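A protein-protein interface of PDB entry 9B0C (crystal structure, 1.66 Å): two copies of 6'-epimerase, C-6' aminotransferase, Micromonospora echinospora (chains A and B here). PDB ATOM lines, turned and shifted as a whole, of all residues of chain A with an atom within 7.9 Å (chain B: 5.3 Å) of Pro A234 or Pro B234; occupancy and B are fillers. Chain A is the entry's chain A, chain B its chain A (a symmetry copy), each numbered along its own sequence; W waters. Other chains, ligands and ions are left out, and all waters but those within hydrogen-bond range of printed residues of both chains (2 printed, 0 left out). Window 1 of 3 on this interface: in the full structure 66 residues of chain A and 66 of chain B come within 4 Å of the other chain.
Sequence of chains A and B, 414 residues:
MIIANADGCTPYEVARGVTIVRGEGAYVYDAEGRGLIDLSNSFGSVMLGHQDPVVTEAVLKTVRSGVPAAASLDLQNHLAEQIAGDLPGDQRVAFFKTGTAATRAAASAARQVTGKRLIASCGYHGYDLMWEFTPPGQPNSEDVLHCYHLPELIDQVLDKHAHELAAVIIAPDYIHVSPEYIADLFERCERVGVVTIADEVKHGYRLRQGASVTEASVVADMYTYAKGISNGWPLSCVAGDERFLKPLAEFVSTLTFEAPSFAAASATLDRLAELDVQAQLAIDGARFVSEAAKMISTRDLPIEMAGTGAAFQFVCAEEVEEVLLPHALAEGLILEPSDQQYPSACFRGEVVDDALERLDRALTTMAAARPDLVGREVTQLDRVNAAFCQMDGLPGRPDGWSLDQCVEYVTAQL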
ATOM      1  N   PHE A  96     -11.443  32.655   8.001  1.00  0.00           N
ATOM      2  CA  PHE A  96     -11.276  32.432   9.434  1.00  0.00           C
ATOM      3  C   PHE A  96     -11.983  31.132   9.795  1.00  0.00           C
ATOM      4  O   PHE A  96     -12.538  30.440   8.929  1.00  0.00           O
ATOM      5  CB  PHE A  96     -11.792  33.641  10.239  1.00  0.00           C
ATOM      6  CG  PHE A  96     -11.017  34.882   9.938  1.00  0.00           C
ATOM      7  CD1 PHE A  96      -9.834  35.142  10.610  1.00  0.00           C
ATOM      8  CD2 PHE A  96     -11.415  35.731   8.908  1.00  0.00           C
ATOM      9  CE1 PHE A  96      -9.060  36.241  10.272  1.00  0.00           C
ATOM     10  CE2 PHE A  96     -10.655  36.831   8.560  1.00  0.00           C
ATOM     11  CZ  PHE A  96      -9.479  37.095   9.248  1.00  0.00           C
ATOM     12  N   LYS A  97     -11.966  30.781  11.073  1.00  0.00           N
ATOM     13  CA  LYS A  97     -12.536  29.502  11.476  1.00  0.00           C
ATOM     14  C   LYS A  97     -13.853  29.625  12.231  1.00  0.00           C
ATOM     15  O   LYS A  97     -14.603  28.648  12.269  1.00  0.00           O
ATOM     16  CB  LYS A  97     -11.528  28.696  12.329  1.00  0.00           C
ATOM     17  CG  LYS A  97     -10.195  28.379  11.614  1.00  0.00           C
ATOM     18  CD  LYS A  97     -10.386  27.705  10.231  1.00  0.00           C
ATOM     19  CE  LYS A  97     -10.349  26.170  10.360  1.00  0.00           C
ATOM     20  NZ  LYS A  97     -11.040  25.438   9.225  1.00  0.00           N
ATOM     21  N   THR A  98     -14.180  30.793  12.799  1.00  0.00           N
ATOM     22  CA  THR A  98     -15.439  31.012  13.497  1.00  0.00           C
ATOM     23  C   THR A  98     -16.023  32.349  13.071  1.00  0.00           C
ATOM     24  O   THR A  98     -15.310  33.206  12.546  1.00  0.00           O
ATOM     25  CB  THR A  98     -15.288  31.048  15.028  1.00  0.00           C
ATOM     26  OG1 THR A  98     -14.467  32.167  15.395  1.00  0.00           O
ATOM     27  CG2 THR A  98     -14.628  29.762  15.562  1.00  0.00           C
ATOM     28  N   GLY A  99     -17.316  32.533  13.345  1.00  0.00           N
ATOM     29  CA  GLY A  99     -17.944  33.820  13.053  1.00  0.00           C
ATOM     30  C   GLY A  99     -17.390  34.945  13.912  1.00  0.00           C
ATOM     31  O   GLY A  99     -17.210  36.074  13.437  1.00  0.00           O
ATOM     32  N   ALA A 226     -20.583  32.819   8.082  1.00  0.00           N
ATOM     33  CA  ALA A 226     -20.110  31.590   8.726  1.00  0.00           C
ATOM     34  C   ALA A 226     -21.135  30.445   8.649  1.00  0.00           C
ATOM     35  O   ALA A 226     -20.872  29.430   7.993  1.00  0.00           O
ATOM     36  CB  ALA A 226     -19.715  31.873  10.178  1.00  0.00           C
ATOM     37  N   ILE A 229     -22.299  28.766   5.026  1.00  0.00           N
ATOM     38  CA  ILE A 229     -21.411  28.446   3.915  1.00  0.00           C
ATOM     39  C   ILE A 229     -20.765  27.066   3.994  1.00  0.00           C
ATOM     40  O   ILE A 229     -20.174  26.631   2.991  1.00  0.00           O
ATOM     41  CB  ILE A 229     -20.316  29.531   3.746  1.00  0.00           C
ATOM     42  CG1 ILE A 229     -19.357  29.533   4.939  1.00  0.00           C
ATOM     43  CG2 ILE A 229     -20.948  30.901   3.515  1.00  0.00           C
ATOM     44  CD1 ILE A 229     -18.134  30.436   4.751  1.00  0.00           C
ATOM     45  N   SER A 230     -20.891  26.337   5.117  1.00  0.00           N
ATOM     46  CA  SER A 230     -20.047  25.155   5.268  1.00  0.00           C
ATOM     47  C   SER A 230     -20.733  23.936   5.882  1.00  0.00           C
ATOM     48  O   SER A 230     -20.032  22.981   6.237  1.00  0.00           O
ATOM     49  CB  SER A 230     -18.807  25.484   6.112  1.00  0.00           C
ATOM     50  OG  SER A 230     -19.197  26.098   7.316  1.00  0.00           O
ATOM     51  N   ASN A 231     -22.056  23.940   6.037  1.00  0.00           N
ATOM     52  CA  ASN A 231     -22.803  22.771   6.523  1.00  0.00           C
ATOM     53  C   ASN A 231     -22.225  22.148   7.792  1.00  0.00           C
ATOM     54  O   ASN A 231     -22.175  20.922   7.936  1.00  0.00           O
ATOM     55  CB  ASN A 231     -22.926  21.697   5.447  1.00  0.00           C
ATOM     56  CG  ASN A 231     -24.235  20.951   5.574  1.00  0.00           C
ATOM     57  OD1 ASN A 231     -25.260  21.584   5.801  1.00  0.00           O
ATOM     58  ND2 ASN A 231     -24.211  19.614   5.457  1.00  0.00           N
ATOM     59  N   GLY A 232     -21.813  22.980   8.741  1.00  0.00           N
ATOM     60  CA  GLY A 232     -21.362  22.462  10.022  1.00  0.00           C
ATOM     61  C   GLY A 232     -19.866  22.292  10.156  1.00  0.00           C
ATOM     62  O   GLY A 232     -19.409  21.731  11.160  1.00  0.00           O
ATOM     63  N   TRP A 233     -19.099  22.743   9.185  1.00  0.00           N
ATOM     64  CA  TRP A 233     -17.650  22.698   9.213  1.00  0.00           C
ATOM     65  C   TRP A 233     -17.103  24.069   9.572  1.00  0.00           C
ATOM     66  O   TRP A 233     -17.696  25.094   9.197  1.00  0.00           O
ATOM     67  CB  TRP A 233     -17.119  22.232   7.854  1.00  0.00           C
ATOM     68  CG  TRP A 233     -17.442  20.770   7.693  1.00  0.00           C
ATOM     69  CD1 TRP A 233     -18.630  20.221   7.264  1.00  0.00           C
ATOM     70  CD2 TRP A 233     -16.593  19.677   8.033  1.00  0.00           C
ATOM     71  NE1 TRP A 233     -18.550  18.849   7.302  1.00  0.00           N
ATOM     72  CE2 TRP A 233     -17.310  18.490   7.766  1.00  0.00           C
ATOM     73  CE3 TRP A 233     -15.287  19.585   8.526  1.00  0.00           C
ATOM     74  CZ2 TRP A 233     -16.762  17.226   7.981  1.00  0.00           C
ATOM     75  CZ3 TRP A 233     -14.740  18.325   8.734  1.00  0.00           C
ATOM     76  CH2 TRP A 233     -15.477  17.167   8.470  1.00  0.00           C
ATOM     77  N   PRO A 234     -16.004  24.134  10.330  1.00  0.00           N
ATOM     78  CA  PRO A 234     -15.589  25.431  10.888  1.00  0.00           C
ATOM     79  C   PRO A 234     -14.870  26.307   9.879  1.00  0.00           C
ATOM     80  O   PRO A 234     -13.638  26.281   9.766  1.00  0.00           O
ATOM     81  CB  PRO A 234     -14.667  25.043  12.046  1.00  0.00           C
ATOM     82  CG  PRO A 234     -14.068  23.725  11.604  1.00  0.00           C
ATOM     83  CD  PRO A 234     -15.161  23.020  10.809  1.00  0.00           C
ATOM     84  N   LEU A 235     -15.641  27.129   9.174  1.00  0.00           N
ATOM     85  CA  LEU A 235     -15.069  28.061   8.223  1.00  0.00           C
ATOM     86  C   LEU A 235     -15.940  29.302   8.177  1.00  0.00           C
ATOM     87  O   LEU A 235     -17.169  29.217   8.214  1.00  0.00           O
ATOM     88  CB  LEU A 235     -14.949  27.438   6.826  1.00  0.00           C
ATOM     89  CG  LEU A 235     -14.054  28.193   5.839  1.00  0.00           C
ATOM     90  CD1 LEU A 235     -12.619  28.206   6.294  1.00  0.00           C
ATOM     91  CD2 LEU A 235     -14.157  27.539   4.449  1.00  0.00           C
ATOM     92  N   SER A 236     -15.292  30.459   8.124  1.00  0.00           N
ATOM     93  CA  SER A 236     -15.971  31.735   8.084  1.00  0.00           C
ATOM     94  C   SER A 236     -15.165  32.645   7.176  1.00  0.00           C
ATOM     95  O   SER A 236     -14.060  32.295   6.760  1.00  0.00           O
ATOM     96  CB  SER A 236     -16.052  32.333   9.487  1.00  0.00           C
ATOM     97  OG  SER A 236     -14.730  32.642   9.916  1.00  0.00           O
ATOM     98  N   LEU A 255      -3.865  26.610  10.769  1.00  0.00           N
ATOM     99  CA  LEU A 255      -4.835  25.777  10.065  1.00  0.00           C
ATOM    100  C   LEU A 255      -5.937  26.599   9.398  1.00  0.00           C
ATOM    101  O   LEU A 255      -7.037  26.090   9.161  1.00  0.00           O
ATOM    102  CB  LEU A 255      -5.438  24.746  11.021  1.00  0.00           C
ATOM    103  CG  LEU A 255      -4.410  23.756  11.570  1.00  0.00           C
ATOM    104  CD1 LEU A 255      -5.044  22.795  12.566  1.00  0.00           C
ATOM    105  CD2 LEU A 255      -3.765  22.960  10.425  1.00  0.00           C
ATOM    106  N   THR A 256      -5.655  27.866   9.070  1.00  0.00           N
ATOM    107  CA  THR A 256      -6.638  28.652   8.318  1.00  0.00           C
ATOM    108  C   THR A 256      -7.060  27.925   7.052  1.00  0.00           C
ATOM    109  O   THR A 256      -8.235  27.955   6.663  1.00  0.00           O
ATOM    110  CB  THR A 256      -6.065  30.018   7.951  1.00  0.00           C
ATOM    111  OG1 THR A 256      -5.949  30.820   9.134  1.00  0.00           O
ATOM    112  CG2 THR A 256      -6.987  30.741   6.960  1.00  0.00           C
ATOM    113  N   GLU A 258      -6.709  24.522   6.341  1.00  0.00           N
ATOM    114  CA  GLU A 258      -6.922  23.078   6.391  1.00  0.00           C
ATOM    115  C   GLU A 258      -7.963  22.701   5.347  1.00  0.00           C
ATOM    116  O   GLU A 258      -8.972  23.393   5.163  1.00  0.00           O
ATOM    117  CB  GLU A 258      -7.364  22.609   7.788  1.00  0.00           C
ATOM    118  CG  GLU A 258      -8.571  23.313   8.364  1.00  0.00           C
ATOM    119  CD  GLU A 258      -9.865  22.490   8.296  1.00  0.00           C
ATOM    120  OE1 GLU A 258      -9.974  21.583   7.440  1.00  0.00           O
ATOM    121  OE2 GLU A 258     -10.797  22.770   9.090  1.00  0.00           O
ATOM    122  N   PRO A 260     -10.153  19.958   4.589  1.00  0.00           N
ATOM    123  CA  PRO A 260     -11.524  19.411   4.677  1.00  0.00           C
ATOM    124  C   PRO A 260     -12.602  20.474   4.799  1.00  0.00           C
ATOM    125  O   PRO A 260     -13.663  20.342   4.178  1.00  0.00           O
ATOM    126  CB  PRO A 260     -11.462  18.520   5.925  1.00  0.00           C
ATOM    127  CG  PRO A 260     -10.041  18.022   5.920  1.00  0.00           C
ATOM    128  CD  PRO A 260      -9.242  19.247   5.507  1.00  0.00           C
ATOM    129  N   SER A 261     -12.372  21.541   5.574  1.00  0.00           N
ATOM    130  CA  SER A 261     -13.423  22.557   5.683  1.00  0.00           C
ATOM    131  C   SER A 261     -13.618  23.322   4.381  1.00  0.00           C
ATOM    132  O   SER A 261     -14.745  23.732   4.073  1.00  0.00           O
ATOM    133  CB  SER A 261     -13.113  23.537   6.823  1.00  0.00           C
ATOM    134  OG  SER A 261     -13.292  22.903   8.081  1.00  0.00           O
ATOM    135  N   PHE A 262     -12.542  23.548   3.613  1.00  0.00           N
ATOM    136  CA  PHE A 262     -12.695  24.183   2.303  1.00  0.00           C
ATOM    137  C   PHE A 262     -13.433  23.275   1.330  1.00  0.00           C
ATOM    138  O   PHE A 262     -14.237  23.753   0.527  1.00  0.00           O
ATOM    139  CB  PHE A 262     -11.335  24.570   1.730  1.00  0.00           C
ATOM    140  CG  PHE A 262     -10.901  25.954   2.131  1.00  0.00           C
ATOM    141  CD1 PHE A 262     -10.251  26.163   3.332  1.00  0.00           C
ATOM    142  CD2 PHE A 262     -11.169  27.037   1.322  1.00  0.00           C
ATOM    143  CE1 PHE A 262      -9.862  27.439   3.723  1.00  0.00           C
ATOM    144  CE2 PHE A 262     -10.787  28.312   1.708  1.00  0.00           C
ATOM    145  CZ  PHE A 262     -10.127  28.495   2.924  1.00  0.00           C
ATOM    146  N   ALA A 264     -15.691  21.044   2.204  1.00  0.00           N
ATOM    147  CA  ALA A 264     -17.079  21.115   2.650  1.00  0.00           C
ATOM    148  C   ALA A 264     -17.753  22.398   2.181  1.00  0.00           C
ATOM    149  O   ALA A 264     -18.897  22.379   1.713  1.00  0.00           O
ATOM    150  CB  ALA A 264     -17.145  21.018   4.174  1.00  0.00           C
ATOM    151  N   ALA A 265     -17.072  23.532   2.324  1.00  0.00           N
ATOM    152  CA  ALA A 265     -17.710  24.804   2.016  1.00  0.00           C
ATOM    153  C   ALA A 265     -17.953  24.965   0.524  1.00  0.00           C
ATOM    154  O   ALA A 265     -19.022  25.419   0.110  1.00  0.00           O
ATOM    155  CB  ALA A 265     -16.855  25.963   2.532  1.00  0.00           C
ATOM    156  N   PHE B  96     -11.305  26.152  21.860  1.00  0.00           N
ATOM    157  CA  PHE B  96     -11.358  27.136  20.783  1.00  0.00           C
ATOM    158  C   PHE B  96     -10.948  26.443  19.491  1.00  0.00           C
ATOM    159  O   PHE B  96     -10.677  25.234  19.467  1.00  0.00           O
ATOM    160  CB  PHE B  96     -10.480  28.358  21.116  1.00  0.00           C
ATOM    161  CG  PHE B  96     -10.964  29.077  22.333  1.00  0.00           C
ATOM    162  CD1 PHE B  96     -11.967  30.026  22.227  1.00  0.00           C
ATOM    163  CD2 PHE B  96     -10.492  28.724  23.595  1.00  0.00           C
ATOM    164  CE1 PHE B  96     -12.487  30.629  23.361  1.00  0.00           C
ATOM    165  CE2 PHE B  96     -11.000  29.317  24.735  1.00  0.00           C
ATOM    166  CZ  PHE B  96     -11.993  30.279  24.621  1.00  0.00           C
ATOM    167  N   LYS B  97     -10.905  27.196  18.400  1.00  0.00           N
ATOM    168  CA  LYS B  97     -10.618  26.581  17.112  1.00  0.00           C
ATOM    169  C   LYS B  97      -9.233  26.909  16.567  1.00  0.00           C
ATOM    170  O   LYS B  97      -8.740  26.160  15.722  1.00  0.00           O
ATOM    171  CB  LYS B  97     -11.687  26.972  16.066  1.00  0.00           C
ATOM    172  CG  LYS B  97     -13.128  26.559  16.438  1.00  0.00           C
ATOM    173  CD  LYS B  97     -13.261  25.058  16.804  1.00  0.00           C
ATOM    174  CE  LYS B  97     -13.651  24.226  15.568  1.00  0.00           C
ATOM    175  NZ  LYS B  97     -13.288  22.757  15.673  1.00  0.00           N
ATOM    176  N   SER B 230      -4.034  17.846  17.905  1.00  0.00           N
ATOM    177  CA  SER B 230      -5.115  17.440  17.011  1.00  0.00           C
ATOM    178  C   SER B 230      -4.677  16.992  15.618  1.00  0.00           C
ATOM    179  O   SER B 230      -5.542  16.844  14.746  1.00  0.00           O
ATOM    180  CB  SER B 230      -6.136  18.574  16.851  1.00  0.00           C
ATOM    181  OG  SER B 230      -5.478  19.764  16.491  1.00  0.00           O
ATOM    182  N   GLY B 232      -3.543  18.303  12.925  1.00  0.00           N
ATOM    183  CA  GLY B 232      -3.959  19.061  11.755  1.00  0.00           C
ATOM    184  C   GLY B 232      -5.427  19.416  11.708  1.00  0.00           C
ATOM    185  O   GLY B 232      -5.890  19.939  10.686  1.00  0.00           O
ATOM    186  N   TRP B 233      -6.168  19.144  12.763  1.00  0.00           N
ATOM    187  CA  TRP B 233      -7.573  19.486  12.873  1.00  0.00           C
ATOM    188  C   TRP B 233      -7.731  20.727  13.736  1.00  0.00           C
ATOM    189  O   TRP B 233      -6.955  20.928  14.684  1.00  0.00           O
ATOM    190  CB  TRP B 233      -8.350  18.304  13.461  1.00  0.00           C
ATOM    191  CG  TRP B 233      -8.406  17.210  12.428  1.00  0.00           C
ATOM    192  CD1 TRP B 233      -7.441  16.266  12.157  1.00  0.00           C
ATOM    193  CD2 TRP B 233      -9.450  17.002  11.479  1.00  0.00           C
ATOM    194  NE1 TRP B 233      -7.843  15.474  11.109  1.00  0.00           N
ATOM    195  CE2 TRP B 233      -9.072  15.902  10.677  1.00  0.00           C
ATOM    196  CE3 TRP B 233     -10.675  17.631  11.237  1.00  0.00           C
ATOM    197  CZ2 TRP B 233      -9.880  15.422   9.646  1.00  0.00           C
ATOM    198  CZ3 TRP B 233     -11.482  17.148  10.213  1.00  0.00           C
ATOM    199  CH2 TRP B 233     -11.079  16.063   9.429  1.00  0.00           C
ATOM    200  N   PRO B 234      -8.690  21.601  13.417  1.00  0.00           N
ATOM    201  CA  PRO B 234      -8.716  22.915  14.080  1.00  0.00           C
ATOM    202  C   PRO B 234      -9.312  22.862  15.475  1.00  0.00           C
ATOM    203  O   PRO B 234     -10.519  23.057  15.667  1.00  0.00           O
ATOM    204  CB  PRO B 234      -9.569  23.771  13.141  1.00  0.00           C
ATOM    205  CG  PRO B 234     -10.512  22.776  12.501  1.00  0.00           C
ATOM    206  CD  PRO B 234      -9.717  21.483  12.363  1.00  0.00           C
ATOM    207  N   LEU B 235      -8.451  22.649  16.465  1.00  0.00           N
ATOM    208  CA  LEU B 235      -8.886  22.639  17.847  1.00  0.00           C
ATOM    209  C   LEU B 235      -7.753  23.155  18.714  1.00  0.00           C
ATOM    210  O   LEU B 235      -6.585  22.836  18.488  1.00  0.00           O
ATOM    211  CB  LEU B 235      -9.308  21.234  18.296  1.00  0.00           C
ATOM    212  CG  LEU B 235     -10.100  21.167  19.604  1.00  0.00           C
ATOM    213  CD1 LEU B 235     -11.430  21.861  19.480  1.00  0.00           C
ATOM    214  CD2 LEU B 235     -10.314  19.694  19.999  1.00  0.00           C
ATOM    215  N   SER B 236      -8.107  23.978  19.693  1.00  0.00           N
ATOM    216  CA  SER B 236      -7.150  24.566  20.605  1.00  0.00           C
ATOM    217  C   SER B 236      -7.811  24.631  21.969  1.00  0.00           C
ATOM    218  O   SER B 236      -9.007  24.368  22.099  1.00  0.00           O
ATOM    219  CB  SER B 236      -6.771  25.970  20.138  1.00  0.00           C
ATOM    220  OG  SER B 236      -7.923  26.799  20.242  1.00  0.00           O
ATOM    221  N   LEU B 255     -19.752  26.360  16.362  1.00  0.00           N
ATOM    222  CA  LEU B 255     -19.095  25.087  16.082  1.00  0.00           C
ATOM    223  C   LEU B 255     -17.910  24.822  17.009  1.00  0.00           C
ATOM    224  O   LEU B 255     -16.998  24.068  16.655  1.00  0.00           O
ATOM    225  CB  LEU B 255     -18.654  25.032  14.618  1.00  0.00           C
ATOM    226  CG  LEU B 255     -19.821  25.087  13.630  1.00  0.00           C
ATOM    227  CD1 LEU B 255     -19.329  25.098  12.190  1.00  0.00           C
ATOM    228  CD2 LEU B 255     -20.763  23.891  13.844  1.00  0.00           C
ATOM    229  N   GLU B 258     -18.007  21.062  17.336  1.00  0.00           N
ATOM    230  CA  GLU B 258     -18.143  20.165  16.190  1.00  0.00           C
ATOM    231  C   GLU B 258     -17.347  18.897  16.466  1.00  0.00           C
ATOM    232  O   GLU B 258     -16.228  18.940  16.993  1.00  0.00           O
ATOM    233  CB  GLU B 258     -17.673  20.826  14.883  1.00  0.00           C
ATOM    234  CG  GLU B 258     -16.275  21.400  14.905  1.00  0.00           C
ATOM    235  CD  GLU B 258     -15.232  20.535  14.184  1.00  0.00           C
ATOM    236  OE1 GLU B 258     -15.441  19.309  14.043  1.00  0.00           O
ATOM    237  OE2 GLU B 258     -14.177  21.081  13.777  1.00  0.00           O
ATOM    238  N   SER B 261     -13.348  17.301  14.949  1.00  0.00           N
ATOM    239  CA  SER B 261     -12.079  17.752  15.527  1.00  0.00           C
ATOM    240  C   SER B 261     -11.854  17.192  16.925  1.00  0.00           C
ATOM    241  O   SER B 261     -10.703  16.941  17.307  1.00  0.00           O
ATOM    242  CB  SER B 261     -12.015  19.286  15.562  1.00  0.00           C
ATOM    243  OG  SER B 261     -11.853  19.803  14.250  1.00  0.00           O
HETATM  244  O   HOH W   1      -8.604  19.269   9.195  1.00  0.00           O
HETATM  245  O   HOH W   2     -17.120  19.545  11.315  1.00  0.00           O
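Pro B234 touches Lys A97.
Gly A232 touches Leu B255.
Trp A233 touches Trp B233.
CB of Pro A234 touches CE of Lys B97, at 3.8 Å.
Pro A234 touches Pro B234 (CG to CG, 3.8 Å).
Pro A234 touches Leu B255.
Glu B258 touches Pro A234.
CD1 of Leu A255 touches C of Gly B232 (3.5 Å).
Leu A255 touches Pro B234 (CD1 to N, 3.9 Å).
Glu A258 touches Pro B234.
Water W2 lies within hydrogen-bond range of O of Gly A232 (3.2 Å) and OE1 of Glu B258 (3.2 Å).
Water W1 bridges O of Gly B232 (3.2 Å) and OE1 of Glu A258 (3.2 Å).
Trp A233 touches its own counterpart, Trp B233.
Trp A233 touches Leu B255, and with the chains exchanged Leu A255 touches Trp B233.
Pro A234 touches its own counterpart, Pro B234.
Pro A234 touches Leu B255, and with the chains exchanged Leu A255 touches Pro B234.
Of the 13 pairs that touch across the chains among the printed residues, 12 have their exchanged pair printed and touching as well.
Of the 21 printed residues of chain A, 7 touch a printed residue of chain B.
Hydrophobic or aromatic side chains of chain A that line the printed part of chain B: Trp A233, Pro A234 and Leu A255.
Of the printed residues of chain B, Gly A232 touches Leu B255 (3.5 Å).
Pro A234 touches four residues of chain B.
Pro B234 touches just these residues of chain A: Lys A97 (3.8 Å), Pro A234 (3.8 Å), Leu A255 (3.9 Å) and Glu A258 (3.4 Å).
Ser B236 touches none of the printed residues of chain A.
Of the printed residues of chain A, Leu B255 touches Gly A232 (3.5 Å), Trp A233 (3.4 Å) and Pro A234 (3.9 Å).
The nearest residue of chain B that does not touch Pro A234 is Ser B261 (5.2 Å).
The nearest residue of chain A that does not touch Pro B234 is Ser A261 (5.2 Å).
NZ of Lys A97 is in hydrogen-bond range of O of Pro A234 (2.8 Å).
O of Thr A98 is in hydrogen-bond range of OG of Ser A236.
The side-chain hydroxyl (OG) of Ser A230 is in hydrogen-bond range of the backbone carbonyl oxygen (O) of Trp A233, at 2.6 Å.
The side-chain amino group (NZ) of Lys B97 lies within salt-bridge range of the side-chain carboxylate (OE2) of Glu B258 (2.7 Å).
The side-chain hydroxyl (OG) of Ser B230 lies within hydrogen-bond range of the backbone carbonyl oxygen (O) of Trp B233 (2.6 Å).
OE2 of Glu B258 sits at hydrogen-bond distance from OG of Ser B261, at 2.7 Å.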
